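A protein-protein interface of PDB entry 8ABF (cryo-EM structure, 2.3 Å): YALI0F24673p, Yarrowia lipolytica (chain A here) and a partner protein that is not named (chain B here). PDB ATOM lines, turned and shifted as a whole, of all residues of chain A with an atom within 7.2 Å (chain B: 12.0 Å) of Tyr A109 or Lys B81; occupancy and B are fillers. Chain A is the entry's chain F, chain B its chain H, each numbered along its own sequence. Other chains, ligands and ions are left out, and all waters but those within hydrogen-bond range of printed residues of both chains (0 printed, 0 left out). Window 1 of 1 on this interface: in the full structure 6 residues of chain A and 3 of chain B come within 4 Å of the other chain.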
ATOM      1  N   GLU A  90      18.212  -9.983  32.121  1.00  0.00           N
ATOM      2  CA  GLU A  90      17.897 -10.988  31.128  1.00  0.00           C
ATOM      3  C   GLU A  90      19.180 -11.617  30.578  1.00  0.00           C
ATOM      4  O   GLU A  90      19.232 -12.834  30.419  1.00  0.00           O
ATOM      5  CB  GLU A  90      16.882 -10.422  30.141  1.00  0.00           C
ATOM      6  CG  GLU A  90      17.178 -10.729  28.697  1.00  0.00           C
ATOM      7  CD  GLU A  90      17.672  -9.507  27.946  1.00  0.00           C
ATOM      8  OE1 GLU A  90      16.939  -8.492  27.944  1.00  0.00           O
ATOM      9  OE2 GLU A  90      18.798  -9.564  27.412  1.00  0.00           O
ATOM     10  N   CYS A  91      20.200 -10.793  30.305  1.00  0.00           N
ATOM     11  CA  CYS A  91      21.484 -11.295  29.836  1.00  0.00           C
ATOM     12  C   CYS A  91      22.047 -12.310  30.830  1.00  0.00           C
ATOM     13  O   CYS A  91      22.436 -13.402  30.432  1.00  0.00           O
ATOM     14  CB  CYS A  91      22.499 -10.180  29.575  1.00  0.00           C
ATOM     15  SG  CYS A  91      24.117 -10.767  28.979  1.00  0.00           S
ATOM     16  N   ARG A  94      20.361 -15.668  30.693  1.00  0.00           N
ATOM     17  CA  ARG A  94      20.741 -16.419  29.502  1.00  0.00           C
ATOM     18  C   ARG A  94      22.109 -17.074  29.672  1.00  0.00           C
ATOM     19  O   ARG A  94      22.263 -18.254  29.363  1.00  0.00           O
ATOM     20  CB  ARG A  94      20.733 -15.560  28.231  1.00  0.00           C
ATOM     21  CG  ARG A  94      19.362 -15.010  27.880  1.00  0.00           C
ATOM     22  CD  ARG A  94      19.323 -14.077  26.692  1.00  0.00           C
ATOM     23  NE  ARG A  94      20.006 -12.798  26.843  1.00  0.00           N
ATOM     24  CZ  ARG A  94      21.047 -12.422  26.108  1.00  0.00           C
ATOM     25  NH1 ARG A  94      21.540 -13.250  25.206  1.00  0.00           N
ATOM     26  NH2 ARG A  94      21.604 -11.232  26.276  1.00  0.00           N
ATOM     27  N   VAL A  95      23.081 -16.295  30.159  1.00  0.00           N
ATOM     28  CA  VAL A  95      24.464 -16.731  30.194  1.00  0.00           C
ATOM     29  C   VAL A  95      24.615 -17.855  31.226  1.00  0.00           C
ATOM     30  O   VAL A  95      25.249 -18.868  30.930  1.00  0.00           O
ATOM     31  CB  VAL A  95      25.432 -15.543  30.401  1.00  0.00           C
ATOM     32  CG1 VAL A  95      26.842 -15.984  30.764  1.00  0.00           C
ATOM     33  CG2 VAL A  95      25.479 -14.635  29.177  1.00  0.00           C
ATOM     34  N   TYR A 104      29.450 -26.732  27.004  1.00  0.00           N
ATOM     35  CA  TYR A 104      29.620 -25.289  27.003  1.00  0.00           C
ATOM     36  C   TYR A 104      31.107 -24.962  26.915  1.00  0.00           C
ATOM     37  O   TYR A 104      31.489 -23.974  26.293  1.00  0.00           O
ATOM     38  CB  TYR A 104      28.975 -24.646  28.236  1.00  0.00           C
ATOM     39  CG  TYR A 104      29.369 -23.205  28.449  1.00  0.00           C
ATOM     40  CD1 TYR A 104      28.812 -22.187  27.686  1.00  0.00           C
ATOM     41  CD2 TYR A 104      30.337 -22.860  29.382  1.00  0.00           C
ATOM     42  CE1 TYR A 104      29.184 -20.863  27.863  1.00  0.00           C
ATOM     43  CE2 TYR A 104      30.730 -21.541  29.563  1.00  0.00           C
ATOM     44  CZ  TYR A 104      30.143 -20.537  28.810  1.00  0.00           C
ATOM     45  OH  TYR A 104      30.521 -19.236  28.997  1.00  0.00           O
ATOM     46  N   HIS A 106      33.343 -26.586  25.380  1.00  0.00           N
ATOM     47  CA  HIS A 106      33.776 -26.808  24.008  1.00  0.00           C
ATOM     48  C   HIS A 106      32.857 -26.066  23.038  1.00  0.00           C
ATOM     49  O   HIS A 106      32.442 -26.624  22.021  1.00  0.00           O
ATOM     50  CB  HIS A 106      33.898 -28.314  23.703  1.00  0.00           C
ATOM     51  CG  HIS A 106      34.944 -29.010  24.511  1.00  0.00           C
ATOM     52  ND1 HIS A 106      36.299 -28.811  24.306  1.00  0.00           N
ATOM     53  CD2 HIS A 106      34.844 -29.886  25.536  1.00  0.00           C
ATOM     54  CE1 HIS A 106      36.986 -29.542  25.163  1.00  0.00           C
ATOM     55  NE2 HIS A 106      36.115 -30.210  25.932  1.00  0.00           N
ATOM     56  N   ALA A 107      32.536 -24.808  23.372  1.00  0.00           N
ATOM     57  CA  ALA A 107      31.778 -23.940  22.484  1.00  0.00           C
ATOM     58  C   ALA A 107      32.708 -22.901  21.866  1.00  0.00           C
ATOM     59  O   ALA A 107      33.770 -22.600  22.409  1.00  0.00           O
ATOM     60  CB  ALA A 107      30.599 -23.318  23.201  1.00  0.00           C
ATOM     61  N   GLU A 108      32.310 -22.400  20.696  1.00  0.00           N
ATOM     62  CA  GLU A 108      33.123 -21.467  19.938  1.00  0.00           C
ATOM     63  C   GLU A 108      32.976 -20.085  20.571  1.00  0.00           C
ATOM     64  O   GLU A 108      33.967 -19.447  20.934  1.00  0.00           O
ATOM     65  CB  GLU A 108      32.705 -21.519  18.465  1.00  0.00           C
ATOM     66  CG  GLU A 108      33.687 -20.851  17.510  1.00  0.00           C
ATOM     67  CD  GLU A 108      33.613 -19.334  17.411  1.00  0.00           C
ATOM     68  OE1 GLU A 108      34.648 -18.675  17.660  1.00  0.00           O
ATOM     69  OE2 GLU A 108      32.530 -18.810  17.073  1.00  0.00           O
ATOM     70  N   TYR A 109      31.715 -19.668  20.718  1.00  0.00           N
ATOM     71  CA  TYR A 109      31.368 -18.362  21.243  1.00  0.00           C
ATOM     72  C   TYR A 109      30.746 -18.503  22.628  1.00  0.00           C
ATOM     73  O   TYR A 109      29.661 -19.070  22.760  1.00  0.00           O
ATOM     74  CB  TYR A 109      30.385 -17.643  20.310  1.00  0.00           C
ATOM     75  CG  TYR A 109      29.876 -16.326  20.840  1.00  0.00           C
ATOM     76  CD1 TYR A 109      30.752 -15.275  21.074  1.00  0.00           C
ATOM     77  CD2 TYR A 109      28.531 -16.124  21.119  1.00  0.00           C
ATOM     78  CE1 TYR A 109      30.308 -14.056  21.563  1.00  0.00           C
ATOM     79  CE2 TYR A 109      28.072 -14.914  21.621  1.00  0.00           C
ATOM     80  CZ  TYR A 109      28.964 -13.875  21.843  1.00  0.00           C
ATOM     81  OH  TYR A 109      28.526 -12.674  22.327  1.00  0.00           O
ATOM     82  N   LYS A 110      31.428 -17.950  23.631  1.00  0.00           N
ATOM     83  CA  LYS A 110      30.862 -17.845  24.967  1.00  0.00           C
ATOM     84  C   LYS A 110      30.456 -16.392  25.226  1.00  0.00           C
ATOM     85  O   LYS A 110      31.311 -15.517  25.351  1.00  0.00           O
ATOM     86  CB  LYS A 110      31.854 -18.397  25.999  1.00  0.00           C
ATOM     87  CG  LYS A 110      32.340 -19.825  25.784  1.00  0.00           C
ATOM     88  CD  LYS A 110      33.455 -20.191  26.748  1.00  0.00           C
ATOM     89  CE  LYS A 110      33.867 -21.650  26.747  1.00  0.00           C
ATOM     90  NZ  LYS A 110      33.835 -22.245  25.390  1.00  0.00           N
ATOM     91  N   GLU A 111      29.144 -16.141  25.321  1.00  0.00           N
ATOM     92  CA  GLU A 111      28.608 -14.821  25.605  1.00  0.00           C
ATOM     93  C   GLU A 111      28.907 -14.414  27.052  1.00  0.00           C
ATOM     94  O   GLU A 111      28.833 -15.242  27.953  1.00  0.00           O
ATOM     95  CB  GLU A 111      27.089 -14.872  25.436  1.00  0.00           C
ATOM     96  CG  GLU A 111      26.467 -13.516  25.148  1.00  0.00           C
ATOM     97  CD  GLU A 111      25.028 -13.378  25.616  1.00  0.00           C
ATOM     98  OE1 GLU A 111      24.643 -12.275  26.080  1.00  0.00           O
ATOM     99  OE2 GLU A 111      24.299 -14.387  25.535  1.00  0.00           O
ATOM    100  N   ASP A 112      29.230 -13.131  27.263  1.00  0.00           N
ATOM    101  CA  ASP A 112      29.245 -12.496  28.580  1.00  0.00           C
ATOM    102  C   ASP A 112      28.180 -11.400  28.647  1.00  0.00           C
ATOM    103  O   ASP A 112      27.403 -11.222  27.713  1.00  0.00           O
ATOM    104  CB  ASP A 112      30.614 -11.901  28.933  1.00  0.00           C
ATOM    105  CG  ASP A 112      31.186 -11.057  27.812  1.00  0.00           C
ATOM    106  OD1 ASP A 112      30.828  -9.873  27.712  1.00  0.00           O
ATOM    107  OD2 ASP A 112      31.945 -11.621  27.009  1.00  0.00           O
ATOM    108  N   CYS A 113      28.150 -10.661  29.765  1.00  0.00           N
ATOM    109  CA  CYS A 113      27.171  -9.604  29.970  1.00  0.00           C
ATOM    110  C   CYS A 113      27.827  -8.259  30.232  1.00  0.00           C
ATOM    111  O   CYS A 113      27.188  -7.349  30.765  1.00  0.00           O
ATOM    112  CB  CYS A 113      26.231  -9.951  31.111  1.00  0.00           C
ATOM    113  SG  CYS A 113      25.203 -11.357  30.632  1.00  0.00           S
ATOM    114  N   VAL A 114      29.080  -8.138  29.797  1.00  0.00           N
ATOM    115  CA  VAL A 114      29.829  -6.925  30.053  1.00  0.00           C
ATOM    116  C   VAL A 114      29.164  -5.745  29.352  1.00  0.00           C
ATOM    117  O   VAL A 114      28.993  -4.695  29.961  1.00  0.00           O
ATOM    118  CB  VAL A 114      31.302  -7.122  29.664  1.00  0.00           C
ATOM    119  CG1 VAL A 114      32.022  -5.804  29.450  1.00  0.00           C
ATOM    120  CG2 VAL A 114      32.014  -7.933  30.722  1.00  0.00           C
ATOM    121  N   GLU A 115      28.735  -5.935  28.103  1.00  0.00           N
ATOM    122  CA  GLU A 115      28.139  -4.842  27.352  1.00  0.00           C
ATOM    123  C   GLU A 115      26.941  -4.259  28.099  1.00  0.00           C
ATOM    124  O   GLU A 115      26.836  -3.041  28.278  1.00  0.00           O
ATOM    125  CB  GLU A 115      27.724  -5.350  25.974  1.00  0.00           C
ATOM    126  CG  GLU A 115      28.396  -4.608  24.843  1.00  0.00           C
ATOM    127  CD  GLU A 115      28.343  -5.359  23.525  1.00  0.00           C
ATOM    128  OE1 GLU A 115      27.241  -5.457  22.950  1.00  0.00           O
ATOM    129  OE2 GLU A 115      29.395  -5.871  23.102  1.00  0.00           O
ATOM    130  N   GLU A 116      26.042  -5.151  28.536  1.00  0.00           N
ATOM    131  CA  GLU A 116      24.815  -4.741  29.199  1.00  0.00           C
ATOM    132  C   GLU A 116      25.124  -4.074  30.536  1.00  0.00           C
ATOM    133  O   GLU A 116      24.427  -3.148  30.964  1.00  0.00           O
ATOM    134  CB  GLU A 116      23.931  -5.951  29.458  1.00  0.00           C
ATOM    135  CG  GLU A 116      23.117  -6.319  28.240  1.00  0.00           C
ATOM    136  CD  GLU A 116      23.759  -7.384  27.377  1.00  0.00           C
ATOM    137  OE1 GLU A 116      23.041  -7.961  26.519  1.00  0.00           O
ATOM    138  OE2 GLU A 116      24.943  -7.701  27.604  1.00  0.00           O
ATOM    139  N   GLU B  73      30.523   5.369  13.716  1.00  0.00           N
ATOM    140  CA  GLU B  73      29.406   4.589  14.224  1.00  0.00           C
ATOM    141  C   GLU B  73      29.504   3.143  13.756  1.00  0.00           C
ATOM    142  O   GLU B  73      29.099   2.240  14.475  1.00  0.00           O
ATOM    143  CB  GLU B  73      28.083   5.160  13.740  1.00  0.00           C
ATOM    144  CG  GLU B  73      27.606   6.338  14.556  1.00  0.00           C
ATOM    145  CD  GLU B  73      26.688   7.291  13.808  1.00  0.00           C
ATOM    146  OE1 GLU B  73      26.335   6.995  12.643  1.00  0.00           O
ATOM    147  OE2 GLU B  73      26.336   8.340  14.387  1.00  0.00           O
ATOM    148  N   LYS B  74      30.009   2.925  12.540  1.00  0.00           N
ATOM    149  CA  LYS B  74      30.131   1.561  12.056  1.00  0.00           C
ATOM    150  C   LYS B  74      31.193   0.836  12.873  1.00  0.00           C
ATOM    151  O   LYS B  74      31.004  -0.315  13.250  1.00  0.00           O
ATOM    152  CB  LYS B  74      30.528   1.528  10.581  1.00  0.00           C
ATOM    153  CG  LYS B  74      30.572   0.139   9.956  1.00  0.00           C
ATOM    154  CD  LYS B  74      29.205  -0.510   9.795  1.00  0.00           C
ATOM    155  CE  LYS B  74      29.183  -1.694   8.848  1.00  0.00           C
ATOM    156  NZ  LYS B  74      29.340  -1.269   7.437  1.00  0.00           N
ATOM    157  N   ASN B  75      32.298   1.538  13.135  1.00  0.00           N
ATOM    158  CA  ASN B  75      33.412   0.958  13.862  1.00  0.00           C
ATOM    159  C   ASN B  75      32.916   0.544  15.235  1.00  0.00           C
ATOM    160  O   ASN B  75      33.207  -0.546  15.696  1.00  0.00           O
ATOM    161  CB  ASN B  75      34.592   1.914  14.016  1.00  0.00           C
ATOM    162  CG  ASN B  75      35.659   1.349  14.931  1.00  0.00           C
ATOM    163  OD1 ASN B  75      35.706   1.694  16.108  1.00  0.00           O
ATOM    164  ND2 ASN B  75      36.491   0.453  14.417  1.00  0.00           N
ATOM    165  N   GLU B  76      32.096   1.397  15.841  1.00  0.00           N
ATOM    166  CA  GLU B  76      31.624   1.109  17.180  1.00  0.00           C
ATOM    167  C   GLU B  76      30.728  -0.127  17.155  1.00  0.00           C
ATOM    168  O   GLU B  76      30.773  -0.932  18.077  1.00  0.00           O
ATOM    169  CB  GLU B  76      30.922   2.330  17.767  1.00  0.00           C
ATOM    170  CG  GLU B  76      30.019   2.016  18.947  1.00  0.00           C
ATOM    171  CD  GLU B  76      29.379   3.212  19.635  1.00  0.00           C
ATOM    172  OE1 GLU B  76      29.923   4.334  19.522  1.00  0.00           O
ATOM    173  OE2 GLU B  76      28.333   3.019  20.294  1.00  0.00           O
ATOM    174  N   TRP B  77      29.918  -0.244  16.106  1.00  0.00           N
ATOM    175  CA  TRP B  77      28.937  -1.307  16.029  1.00  0.00           C
ATOM    176  C   TRP B  77      29.613  -2.642  15.743  1.00  0.00           C
ATOM    177  O   TRP B  77      29.148  -3.683  16.196  1.00  0.00           O
ATOM    178  CB  TRP B  77      27.894  -0.964  14.970  1.00  0.00           C
ATOM    179  CG  TRP B  77      26.875  -2.047  14.848  1.00  0.00           C
ATOM    180  CD1 TRP B  77      25.800  -2.256  15.664  1.00  0.00           C
ATOM    181  CD2 TRP B  77      26.853  -3.097  13.871  1.00  0.00           C
ATOM    182  NE1 TRP B  77      25.094  -3.351  15.252  1.00  0.00           N
ATOM    183  CE2 TRP B  77      25.722  -3.893  14.162  1.00  0.00           C
ATOM    184  CE3 TRP B  77      27.682  -3.442  12.797  1.00  0.00           C
ATOM    185  CZ2 TRP B  77      25.401  -5.021  13.411  1.00  0.00           C
ATOM    186  CZ3 TRP B  77      27.361  -4.558  12.053  1.00  0.00           C
ATOM    187  CH2 TRP B  77      26.228  -5.322  12.353  1.00  0.00           C
ATOM    188  N   LEU B  78      30.703  -2.605  14.981  1.00  0.00           N
ATOM    189  CA  LEU B  78      31.371  -3.840  14.611  1.00  0.00           C
ATOM    190  C   LEU B  78      31.990  -4.501  15.842  1.00  0.00           C
ATOM    191  O   LEU B  78      32.248  -5.697  15.827  1.00  0.00           O
ATOM    192  CB  LEU B  78      32.474  -3.513  13.604  1.00  0.00           C
ATOM    193  CG  LEU B  78      32.033  -3.276  12.163  1.00  0.00           C
ATOM    194  CD1 LEU B  78      33.205  -2.780  11.332  1.00  0.00           C
ATOM    195  CD2 LEU B  78      31.456  -4.548  11.564  1.00  0.00           C
ATOM    196  N   TYR B  79      32.300  -3.704  16.874  1.00  0.00           N
ATOM    197  CA  TYR B  79      32.968  -4.215  18.063  1.00  0.00           C
ATOM    198  C   TYR B  79      31.987  -4.422  19.208  1.00  0.00           C
ATOM    199  O   TYR B  79      32.392  -4.487  20.364  1.00  0.00           O
ATOM    200  CB  TYR B  79      34.142  -3.315  18.452  1.00  0.00           C
ATOM    201  CG  TYR B  79      35.305  -3.496  17.516  1.00  0.00           C
ATOM    202  CD1 TYR B  79      36.301  -4.418  17.800  1.00  0.00           C
ATOM    203  CD2 TYR B  79      35.372  -2.811  16.307  1.00  0.00           C
ATOM    204  CE1 TYR B  79      37.362  -4.622  16.933  1.00  0.00           C
ATOM    205  CE2 TYR B  79      36.418  -3.015  15.418  1.00  0.00           C
ATOM    206  CZ  TYR B  79      37.418  -3.920  15.739  1.00  0.00           C
ATOM    207  OH  TYR B  79      38.455  -4.138  14.881  1.00  0.00           O
ATOM    208  N   THR B  80      30.700  -4.510  18.884  1.00  0.00           N
ATOM    209  CA  THR B  80      29.715  -4.980  19.846  1.00  0.00           C
ATOM    210  C   THR B  80      29.437  -6.450  19.562  1.00  0.00           C
ATOM    211  O   THR B  80      29.990  -6.997  18.612  1.00  0.00           O
ATOM    212  CB  THR B  80      28.449  -4.123  19.786  1.00  0.00           C
ATOM    213  OG1 THR B  80      27.859  -4.242  18.491  1.00  0.00           O
ATOM    214  CG2 THR B  80      28.724  -2.670  20.091  1.00  0.00           C
ATOM    215  N   LYS B  81      28.597  -7.070  20.397  1.00  0.00           N
ATOM    216  CA  LYS B  81      28.193  -8.459  20.246  1.00  0.00           C
ATOM    217  C   LYS B  81      27.403  -8.628  18.956  1.00  0.00           C
ATOM    218  O   LYS B  81      27.589  -9.597  18.226  1.00  0.00           O
ATOM    219  CB  LYS B  81      27.150  -8.819  21.303  1.00  0.00           C
ATOM    220  CG  LYS B  81      27.657  -9.077  22.705  1.00  0.00           C
ATOM    221  CD  LYS B  81      26.525  -8.952  23.698  1.00  0.00           C
ATOM    222  CE  LYS B  81      26.704  -9.847  24.898  1.00  0.00           C
ATOM    223  NZ  LYS B  81      25.594  -9.685  25.866  1.00  0.00           N
ATOM    224  N   ALA B  82      26.478  -7.692  18.724  1.00  0.00           N
ATOM    225  CA  ALA B  82      25.624  -7.681  17.546  1.00  0.00           C
ATOM    226  C   ALA B  82      26.442  -7.644  16.253  1.00  0.00           C
ATOM    227  O   ALA B  82      25.996  -8.149  15.219  1.00  0.00           O
ATOM    228  CB  ALA B  82      24.685  -6.508  17.639  1.00  0.00           C
ATOM    229  N   GLY B  83      27.638  -7.043  16.312  1.00  0.00           N
ATOM    230  CA  GLY B  83      28.427  -6.837  15.107  1.00  0.00           C
ATOM    231  C   GLY B  83      29.508  -7.892  14.885  1.00  0.00           C
ATOM    232  O   GLY B  83      30.404  -7.681  14.062  1.00  0.00           O
ATOM    233  N   ARG B  84      29.421  -8.993  15.643  1.00  0.00           N
ATOM    234  CA  ARG B  84      30.403 -10.065  15.675  1.00  0.00           C
ATOM    235  C   ARG B  84      30.679 -10.609  14.281  1.00  0.00           C
ATOM    236  O   ARG B  84      31.832 -10.840  13.916  1.00  0.00           O
ATOM    237  CB  ARG B  84      29.795 -11.268  16.385  1.00  0.00           C
ATOM    238  CG  ARG B  84      30.134 -11.333  17.861  1.00  0.00           C
ATOM    239  CD  ARG B  84      29.885 -12.746  18.287  1.00  0.00           C
ATOM    240  NE  ARG B  84      28.463 -13.012  18.345  1.00  0.00           N
ATOM    241  CZ  ARG B  84      27.948 -14.207  18.125  1.00  0.00           C
ATOM    242  NH1 ARG B  84      28.746 -15.219  17.835  1.00  0.00           N
ATOM    243  NH2 ARG B  84      26.644 -14.385  18.194  1.00  0.00           N
ATOM    244  N   HIS B  85      29.586 -10.879  13.564  1.00  0.00           N
ATOM    245  CA  HIS B  85      29.633 -11.624  12.323  1.00  0.00           C
ATOM    246  C   HIS B  85      30.181 -10.737  11.222  1.00  0.00           C
ATOM    247  O   HIS B  85      30.977 -11.184  10.402  1.00  0.00           O
ATOM    248  CB  HIS B  85      28.233 -12.089  11.934  1.00  0.00           C
ATOM    249  CG  HIS B  85      27.608 -12.936  12.979  1.00  0.00           C
ATOM    250  ND1 HIS B  85      28.155 -14.141  13.370  1.00  0.00           N
ATOM    251  CD2 HIS B  85      26.502 -12.752  13.728  1.00  0.00           C
ATOM    252  CE1 HIS B  85      27.400 -14.673  14.308  1.00  0.00           C
ATOM    253  NE2 HIS B  85      26.381 -13.838  14.546  1.00  0.00           N
ATOM    254  N   GLU B  86      29.689  -9.495  11.204  1.00  0.00           N
ATOM    255  CA  GLU B  86      30.123  -8.492  10.252  1.00  0.00           C
ATOM    256  C   GLU B  86      31.583  -8.140  10.525  1.00  0.00           C
ATOM    257  O   GLU B  86      32.295  -7.805   9.585  1.00  0.00           O
ATOM    258  CB  GLU B  86      29.240  -7.245  10.287  1.00  0.00           C
ATOM    259  CG  GLU B  86      27.854  -7.432   9.690  1.00  0.00           C
ATOM    260  CD  GLU B  86      26.863  -8.284  10.472  1.00  0.00           C
ATOM    261  OE1 GLU B  86      26.997  -8.382  11.717  1.00  0.00           O
ATOM    262  OE2 GLU B  86      25.963  -8.862   9.831  1.00  0.00           O
ATOM    263  N   LEU B  87      32.016  -8.192  11.796  1.00  0.00           N
ATOM    264  CA  LEU B  87      33.423  -7.924  12.085  1.00  0.00           C
ATOM    265  C   LEU B  87      34.301  -9.052  11.550  1.00  0.00           C
ATOM    266  O   LEU B  87      35.422  -8.808  11.109  1.00  0.00           O
ATOM    267  CB  LEU B  87      33.692  -7.691  13.580  1.00  0.00           C
ATOM    268  CG  LEU B  87      35.159  -7.458  13.984  1.00  0.00           C
ATOM    269  CD1 LEU B  87      35.724  -6.158  13.411  1.00  0.00           C
ATOM    270  CD2 LEU B  87      35.328  -7.469  15.499  1.00  0.00           C
ATOM    271  N   ALA B  88      33.793 -10.279  11.629  1.00  0.00           N
ATOM    272  CA  ALA B  88      34.575 -11.445  11.256  1.00  0.00           C
ATOM    273  C   ALA B  88      34.879 -11.405   9.761  1.00  0.00           C
ATOM    274  O   ALA B  88      35.969 -11.781   9.341  1.00  0.00           O
ATOM    275  CB  ALA B  88      33.816 -12.689  11.636  1.00  0.00           C
ATOM    276  N   LYS B  89      33.883 -10.951   8.988  1.00  0.00           N
ATOM    277  CA  LYS B  89      33.969 -10.810   7.542  1.00  0.00           C
ATOM    278  C   LYS B  89      34.887  -9.647   7.170  1.00  0.00           C
ATOM    279  O   LYS B  89      35.654  -9.749   6.210  1.00  0.00           O
ATOM    280  CB  LYS B  89      32.588 -10.517   6.954  1.00  0.00           C
ATOM    281  CG  LYS B  89      31.600 -11.668   6.993  1.00  0.00           C
ATOM    282  CD  LYS B  89      30.227 -11.242   6.521  1.00  0.00           C
ATOM    283  CE  LYS B  89      29.107 -12.101   7.072  1.00  0.00           C
ATOM    284  NZ  LYS B  89      27.806 -11.389   7.066  1.00  0.00           N
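The side-chain sulfur of Cys A91 lies close to the guanidinium group of Arg A94 (3.7 Å). The side-chain sulfur of Cys A113 is disulfide-bonded to the side-chain sulfur of Cys A91 (2.1 Å). NH1 of Arg A94 lies within salt-bridge range of OE2 of Glu A111 (3.0 Å). NH2 of Arg A94 is in salt-bridge range of OE1 of Glu A116, 3.6 Å away. The backbone NH (N) of Val A114 lies within hydrogen-bond range of the side-chain carboxylate (OD1) of Asp A112, at 3.2 Å. OG1 of Thr B80 lies within hydrogen-bond range of O of Trp B77, at 2.7 Å.
CG of Lys B81 touches OH of Tyr A109, 3.7 Å away. Arg B84 touches Tyr A109. Glu A115 touches Thr B80.
Of chain B, only Lys B81 comes within 4 Å of Cys A91. No residue of chain B comes within 4 Å of Ala A107. Tyr A109 touches just these residues of chain B: Lys B81 (3.7 Å) and Arg B84 (3.4 Å). Lys A110 touches none of the printed residues of chain B. Of the printed residues of chain B, Glu A111 touches Lys B81. Asp A112 touches just one residue of chain B: Lys B81 (3.0 Å). No residue of chain B comes within 4 Å of Cys A113. Glu A115 touches two residues of chain B. Of the printed residues of chain B, Glu A116 touches Lys B81 (2.7 Å). Of the printed residues of chain A, Thr B80 touches Glu A115 (3.4 Å). Lys B81 touches just these residues of chain A: Cys A91, Tyr A109, Glu A111, Asp A112, Glu A115 and Glu A116. Printed residues of chain A within 4 Å of Arg B84: Tyr A109. Glu B86 touches none of the printed residues of chain A. The nearest residue of chain B that does not touch Tyr A109 is Ala B82 (6.5 Å).
SG of Cys A91 is in hydrogen-bond range of NZ of Lys B81. The side-chain carboxylate of Glu A111 is in salt-bridge range of the side-chain amino group of Lys B81, 2.8 Å away. The backbone carbonyl oxygen of Asp A112 is in hydrogen-bond range of the side-chain amino group of Lys B81 (3.0 Å). The backbone NH (N) of Lys B81 sits at hydrogen-bond distance from the side-chain carboxylate (OE2) of Glu A115 (3.1 Å). OE2 of Glu A116 lies within salt-bridge range of NZ of Lys B81 (2.7 Å).
Of the 16 printed residues of chain A, 6 touch a printed residue of chain B. Printed residues of chain A that touch a printed residue of chain B: Cys A91, Tyr A109, Glu A111, Asp A112, Glu A115 and Glu A116. Hydrophobic or aromatic side chains of chain A that line the printed part of chain B: Tyr A109. Of the 17 printed residues of chain B, 3 touch a printed residue of chain A. Printed residues of chain B that touch a printed residue of chain A: Thr B80, Lys B81 and Arg B84. Among the printed residues, Asp or Glu carboxylates within 4 Å of a Lys or Arg side-chain nitrogen of the other chain: Glu A111 with Lys B81 and Glu A116 with Lys B81.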
